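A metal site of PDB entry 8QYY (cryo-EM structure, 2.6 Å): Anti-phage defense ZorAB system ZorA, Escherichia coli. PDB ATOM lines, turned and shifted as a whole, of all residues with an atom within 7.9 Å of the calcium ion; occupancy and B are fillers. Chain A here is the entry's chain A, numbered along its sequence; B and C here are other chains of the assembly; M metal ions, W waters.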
ATOM      1  N   HIS A  82       9.899   0.218 -17.755  1.00  0.00           N
ATOM      2  CA  HIS A  82      11.136   0.224 -16.982  1.00  0.00           C
ATOM      3  C   HIS A  82      10.882   0.633 -15.542  1.00  0.00           C
ATOM      4  O   HIS A  82      11.452   0.051 -14.610  1.00  0.00           O
ATOM      5  CB  HIS A  82      12.164   1.149 -17.640  1.00  0.00           C
ATOM      6  CG  HIS A  82      13.369   1.397 -16.802  1.00  0.00           C
ATOM      7  ND1 HIS A  82      14.352   0.448 -16.614  1.00  0.00           N
ATOM      8  CD2 HIS A  82      13.764   2.493 -16.105  1.00  0.00           C
ATOM      9  CE1 HIS A  82      15.298   0.945 -15.842  1.00  0.00           C
ATOM     10  NE2 HIS A  82      14.963   2.179 -15.503  1.00  0.00           N
ATOM     11  N   ASN A  85       9.381  -2.283 -13.730  1.00  0.00           N
ATOM     12  CA  ASN A  85      10.364  -3.330 -13.464  1.00  0.00           C
ATOM     13  C   ASN A  85      11.236  -2.958 -12.262  1.00  0.00           C
ATOM     14  O   ASN A  85      11.451  -3.780 -11.361  1.00  0.00           O
ATOM     15  CB  ASN A  85      11.227  -3.572 -14.707  1.00  0.00           C
ATOM     16  CG  ASN A  85      10.473  -4.297 -15.798  1.00  0.00           C
ATOM     17  OD1 ASN A  85       9.499  -5.001 -15.532  1.00  0.00           O
ATOM     18  ND2 ASN A  85      10.927  -4.136 -17.038  1.00  0.00           N
ATOM     19  N   GLU A  86      11.707  -1.714 -12.220  1.00  0.00           N
ATOM     20  CA  GLU A  86      12.527  -1.276 -11.093  1.00  0.00           C
ATOM     21  C   GLU A  86      11.724  -1.270  -9.798  1.00  0.00           C
ATOM     22  O   GLU A  86      12.230  -1.687  -8.743  1.00  0.00           O
ATOM     23  CB  GLU A  86      13.102   0.103 -11.383  1.00  0.00           C
ATOM     24  CG  GLU A  86      13.981   0.144 -12.609  1.00  0.00           C
ATOM     25  CD  GLU A  86      15.090  -0.887 -12.560  1.00  0.00           C
ATOM     26  OE1 GLU A  86      15.784  -0.954 -11.533  1.00  0.00           O
ATOM     27  OE2 GLU A  86      15.266  -1.626 -13.548  1.00  0.00           O
ATOM     28  N   PHE A  87      10.477  -0.807  -9.842  1.00  0.00           N
ATOM     29  CA  PHE A  87       9.644  -0.779  -8.652  1.00  0.00           C
ATOM     30  C   PHE A  87       9.380  -2.191  -8.137  1.00  0.00           C
ATOM     31  O   PHE A  87       9.426  -2.432  -6.922  1.00  0.00           O
ATOM     32  CB  PHE A  87       8.340  -0.048  -8.953  1.00  0.00           C
ATOM     33  CG  PHE A  87       7.404   0.028  -7.787  1.00  0.00           C
ATOM     34  CD1 PHE A  87       7.797   0.627  -6.613  1.00  0.00           C
ATOM     35  CD2 PHE A  87       6.118  -0.482  -7.877  1.00  0.00           C
ATOM     36  CE1 PHE A  87       6.929   0.711  -5.546  1.00  0.00           C
ATOM     37  CE2 PHE A  87       5.258  -0.399  -6.815  1.00  0.00           C
ATOM     38  CZ  PHE A  87       5.660   0.198  -5.647  1.00  0.00           C
ATOM     39  N   GLU A  89      11.339  -4.671  -8.545  1.00  0.00           N
ATOM     40  CA  GLU A  89      12.583  -5.048  -7.881  1.00  0.00           C
ATOM     41  C   GLU A  89      12.613  -4.504  -6.458  1.00  0.00           C
ATOM     42  O   GLU A  89      13.132  -5.164  -5.550  1.00  0.00           O
ATOM     43  CB  GLU A  89      13.791  -4.551  -8.664  1.00  0.00           C
ATOM     44  CG  GLU A  89      13.987  -5.217 -10.007  1.00  0.00           C
ATOM     45  CD  GLU A  89      15.190  -4.670 -10.735  1.00  0.00           C
ATOM     46  OE1 GLU A  89      15.786  -3.685 -10.241  1.00  0.00           O
ATOM     47  OE2 GLU A  89      15.533  -5.206 -11.808  1.00  0.00           O
ATOM     48  N   SER A  90      12.094  -3.291  -6.250  1.00  0.00           N
ATOM     49  CA  SER A  90      12.101  -2.733  -4.903  1.00  0.00           C
ATOM     50  C   SER A  90      11.179  -3.492  -3.955  1.00  0.00           C
ATOM     51  O   SER A  90      11.456  -3.561  -2.756  1.00  0.00           O
ATOM     52  CB  SER A  90      11.702  -1.258  -4.939  1.00  0.00           C
ATOM     53  OG  SER A  90      10.321  -1.116  -5.209  1.00  0.00           O
ATOM     54  N   PHE A 116      10.713   5.544  -8.578  1.00  0.00           N
ATOM     55  CA  PHE A 116      10.850   4.957  -9.900  1.00  0.00           C
ATOM     56  C   PHE A 116       9.896   5.555 -10.908  1.00  0.00           C
ATOM     57  O   PHE A 116      10.257   5.726 -12.071  1.00  0.00           O
ATOM     58  CB  PHE A 116      10.637   3.438  -9.817  1.00  0.00           C
ATOM     59  CG  PHE A 116      11.379   2.798  -8.681  1.00  0.00           C
ATOM     60  CD1 PHE A 116      12.712   2.466  -8.813  1.00  0.00           C
ATOM     61  CD2 PHE A 116      10.749   2.565  -7.474  1.00  0.00           C
ATOM     62  CE1 PHE A 116      13.391   1.892  -7.771  1.00  0.00           C
ATOM     63  CE2 PHE A 116      11.433   1.996  -6.425  1.00  0.00           C
ATOM     64  CZ  PHE A 116      12.750   1.650  -6.578  1.00  0.00           C
ATOM     65  N   ARG B 108      23.732  -8.125  -7.865  1.00  0.00           N
ATOM     66  CA  ARG B 108      22.610  -7.339  -7.382  1.00  0.00           C
ATOM     67  C   ARG B 108      22.999  -5.869  -7.313  1.00  0.00           C
ATOM     68  O   ARG B 108      24.138  -5.526  -7.005  1.00  0.00           O
ATOM     69  CB  ARG B 108      22.165  -7.813  -6.003  1.00  0.00           C
ATOM     70  CG  ARG B 108      21.958  -9.309  -5.897  1.00  0.00           C
ATOM     71  CD  ARG B 108      20.760  -9.753  -6.698  1.00  0.00           C
ATOM     72  NE  ARG B 108      19.517  -9.167  -6.207  1.00  0.00           N
ATOM     73  CZ  ARG B 108      18.726  -9.720  -5.306  1.00  0.00           C
ATOM     74  NH1 ARG B 108      19.021 -10.889  -4.759  1.00  0.00           N
ATOM     75  NH2 ARG B 108      17.608  -9.097  -4.946  1.00  0.00           N
ATOM     76  N   ALA B 109      22.038  -5.007  -7.615  1.00  0.00           N
ATOM     77  CA  ALA B 109      22.245  -3.566  -7.560  1.00  0.00           C
ATOM     78  C   ALA B 109      21.818  -3.043  -6.190  1.00  0.00           C
ATOM     79  O   ALA B 109      20.716  -3.333  -5.732  1.00  0.00           O
ATOM     80  CB  ALA B 109      21.461  -2.861  -8.664  1.00  0.00           C
ATOM     81  N   ALA B 111      22.442   0.457  -5.471  1.00  0.00           N
ATOM     82  CA  ALA B 111      22.135   1.857  -5.736  1.00  0.00           C
ATOM     83  C   ALA B 111      21.768   2.012  -7.203  1.00  0.00           C
ATOM     84  O   ALA B 111      22.237   1.230  -8.045  1.00  0.00           O
ATOM     85  CB  ALA B 111      23.318   2.770  -5.394  1.00  0.00           C
ATOM     86  N   PRO B 112      20.936   2.986  -7.534  1.00  0.00           N
ATOM     87  CA  PRO B 112      20.615   3.222  -8.948  1.00  0.00           C
ATOM     88  C   PRO B 112      21.839   3.683  -9.719  1.00  0.00           C
ATOM     89  O   PRO B 112      22.727   4.355  -9.185  1.00  0.00           O
ATOM     90  CB  PRO B 112      19.537   4.313  -8.890  1.00  0.00           C
ATOM     91  CG  PRO B 112      19.750   4.979  -7.583  1.00  0.00           C
ATOM     92  CD  PRO B 112      20.219   3.916  -6.645  1.00  0.00           C
ATOM     93  N   THR B 213      21.158   5.187 -18.397  1.00  0.00           N
ATOM     94  CA  THR B 213      21.103   4.681 -17.020  1.00  0.00           C
ATOM     95  C   THR B 213      19.971   3.678 -16.838  1.00  0.00           C
ATOM     96  O   THR B 213      20.090   2.759 -16.027  1.00  0.00           O
ATOM     97  CB  THR B 213      20.956   5.828 -16.023  1.00  0.00           C
ATOM     98  OG1 THR B 213      19.791   6.600 -16.340  1.00  0.00           O
ATOM     99  CG2 THR B 213      22.168   6.727 -16.058  1.00  0.00           C
ATOM    100  N   ALA B 214      18.860   3.853 -17.569  1.00  0.00           N
ATOM    101  CA  ALA B 214      17.806   2.852 -17.545  1.00  0.00           C
ATOM    102  C   ALA B 214      18.295   1.524 -18.105  1.00  0.00           C
ATOM    103  O   ALA B 214      17.961   0.451 -17.588  1.00  0.00           O
ATOM    104  CB  ALA B 214      16.595   3.343 -18.334  1.00  0.00           C
ATOM    105  N   ALA B 215      19.086   1.573 -19.173  1.00  0.00           N
ATOM    106  CA  ALA B 215      19.689   0.353 -19.693  1.00  0.00           C
ATOM    107  C   ALA B 215      20.607  -0.293 -18.656  1.00  0.00           C
ATOM    108  O   ALA B 215      20.581  -1.515 -18.481  1.00  0.00           O
ATOM    109  CB  ALA B 215      20.460   0.653 -20.977  1.00  0.00           C
ATOM    110  N   LEU B 216      21.414   0.513 -17.964  1.00  0.00           N
ATOM    111  CA  LEU B 216      22.281  -0.043 -16.933  1.00  0.00           C
ATOM    112  C   LEU B 216      21.476  -0.568 -15.745  1.00  0.00           C
ATOM    113  O   LEU B 216      21.817  -1.612 -15.173  1.00  0.00           O
ATOM    114  CB  LEU B 216      23.280   1.015 -16.463  1.00  0.00           C
ATOM    115  CG  LEU B 216      24.688   0.902 -17.044  1.00  0.00           C
ATOM    116  CD1 LEU B 216      25.581   1.908 -16.392  1.00  0.00           C
ATOM    117  CD2 LEU B 216      25.228  -0.508 -16.862  1.00  0.00           C
ATOM    118  N   ASP B 217      20.414   0.138 -15.354  1.00  0.00           N
ATOM    119  CA  ASP B 217      19.602  -0.297 -14.233  1.00  0.00           C
ATOM    120  C   ASP B 217      18.901  -1.619 -14.501  1.00  0.00           C
ATOM    121  O   ASP B 217      18.624  -2.374 -13.558  1.00  0.00           O
ATOM    122  CB  ASP B 217      18.567   0.769 -13.881  1.00  0.00           C
ATOM    123  CG  ASP B 217      19.103   1.822 -12.939  1.00  0.00           C
ATOM    124  OD1 ASP B 217      20.078   1.523 -12.223  1.00  0.00           O
ATOM    125  OD2 ASP B 217      18.544   2.931 -12.899  1.00  0.00           O
ATOM    126  N   SER B 218      18.612  -1.914 -15.766  1.00  0.00           N
ATOM    127  CA  SER B 218      17.867  -3.123 -16.089  1.00  0.00           C
ATOM    128  C   SER B 218      18.716  -4.378 -15.983  1.00  0.00           C
ATOM    129  O   SER B 218      18.162  -5.485 -15.925  1.00  0.00           O
ATOM    130  CB  SER B 218      17.291  -3.012 -17.499  1.00  0.00           C
ATOM    131  OG  SER B 218      18.279  -3.275 -18.470  1.00  0.00           O
ATOM    132  N   LEU B 219      20.038  -4.246 -15.957  1.00  0.00           N
ATOM    133  CA  LEU B 219      20.902  -5.428 -15.937  1.00  0.00           C
ATOM    134  C   LEU B 219      20.875  -6.124 -14.586  1.00  0.00           C
ATOM    135  O   LEU B 219      21.076  -7.349 -14.522  1.00  0.00           O
ATOM    136  CB  LEU B 219      22.328  -5.043 -16.304  1.00  0.00           C
ATOM    137  CG  LEU B 219      22.644  -4.720 -17.757  1.00  0.00           C
ATOM    138  CD1 LEU B 219      24.113  -4.404 -17.915  1.00  0.00           C
ATOM    139  CD2 LEU B 219      22.257  -5.869 -18.651  1.00  0.00           C
ATOM    140  N   TYR B 220      20.638  -5.394 -13.505  1.00  0.00           N
ATOM    141  CA  TYR B 220      20.817  -5.915 -12.153  1.00  0.00           C
ATOM    142  C   TYR B 220      19.581  -5.644 -11.324  1.00  0.00           C
ATOM    143  O   TYR B 220      18.839  -4.690 -11.569  1.00  0.00           O
ATOM    144  CB  TYR B 220      22.051  -5.301 -11.502  1.00  0.00           C
ATOM    145  CG  TYR B 220      23.293  -5.473 -12.342  1.00  0.00           C
ATOM    146  CD1 TYR B 220      23.901  -6.706 -12.464  1.00  0.00           C
ATOM    147  CD2 TYR B 220      23.846  -4.399 -13.024  1.00  0.00           C
ATOM    148  CE1 TYR B 220      25.024  -6.876 -13.232  1.00  0.00           C
ATOM    149  CE2 TYR B 220      24.967  -4.559 -13.796  1.00  0.00           C
ATOM    150  CZ  TYR B 220      25.560  -5.798 -13.902  1.00  0.00           C
ATOM    151  OH  TYR B 220      26.688  -5.963 -14.663  1.00  0.00           O
ATOM    152  N   ASP B 221      19.361  -6.508 -10.325  1.00  0.00           N
ATOM    153  CA  ASP B 221      18.182  -6.472  -9.486  1.00  0.00           C
ATOM    154  C   ASP B 221      18.546  -5.984  -8.093  1.00  0.00           C
ATOM    155  O   ASP B 221      19.654  -6.228  -7.610  1.00  0.00           O
ATOM    156  CB  ASP B 221      17.522  -7.846  -9.402  1.00  0.00           C
ATOM    157  CG  ASP B 221      16.791  -8.222 -10.664  1.00  0.00           C
ATOM    158  OD1 ASP B 221      17.251  -7.830 -11.762  1.00  0.00           O
ATOM    159  OD2 ASP B 221      15.753  -8.903 -10.576  1.00  0.00           O
ATOM    160  N   SER B 222      17.604  -5.304  -7.438  1.00  0.00           N
ATOM    161  CA  SER B 222      17.808  -4.758  -6.118  1.00  0.00           C
ATOM    162  C   SER B 222      17.104  -5.619  -5.070  1.00  0.00           C
ATOM    163  O   SER B 222      16.587  -6.694  -5.368  1.00  0.00           O
ATOM    164  CB  SER B 222      17.312  -3.317  -6.073  1.00  0.00           C
ATOM    165  OG  SER B 222      17.894  -2.558  -7.120  1.00  0.00           O
ATOM    166  N   PHE C   6      17.387   4.047  -3.083  1.00  0.00           N
ATOM    167  CA  PHE C   6      16.419   4.314  -4.133  1.00  0.00           C
ATOM    168  C   PHE C   6      15.344   5.263  -3.594  1.00  0.00           C
ATOM    169  O   PHE C   6      14.203   4.903  -3.328  1.00  0.00           O
ATOM    170  CB  PHE C   6      15.808   3.018  -4.655  1.00  0.00           C
ATOM    171  CG  PHE C   6      16.823   2.063  -5.229  1.00  0.00           C
ATOM    172  CD1 PHE C   6      17.581   1.248  -4.400  1.00  0.00           C
ATOM    173  CD2 PHE C   6      17.016   1.976  -6.594  1.00  0.00           C
ATOM    174  CE1 PHE C   6      18.501   0.383  -4.919  1.00  0.00           C
ATOM    175  CE2 PHE C   6      17.944   1.110  -7.118  1.00  0.00           C
ATOM    176  CZ  PHE C   6      18.693   0.305  -6.288  1.00  0.00           C
HETATM  177 CA    CA M   1      17.287  -3.130 -11.825  1.00  0.00          CA
HETATM  178  O   HOH W   1      18.803  -1.793 -10.881  1.00  0.00           O
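The calcium ion is bound by the backbone carbonyl oxygen (O) of Tyr 220 of chain B (2.2 Å), water W1 (2.2 Å), the side-chain carboxylate (OE1) of Glu 89 (2.3 Å), the backbone carbonyl oxygen (O) of Asp 217 of chain B (2.3 Å), the side-chain carboxylate (OE1) of Glu 86 (2.7 Å) and the side-chain carboxylate (OE2) of Glu 89 (2.7 Å).
Slightly farther from the calcium ion lies OE2 of Glu 86 (3.1 Å).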
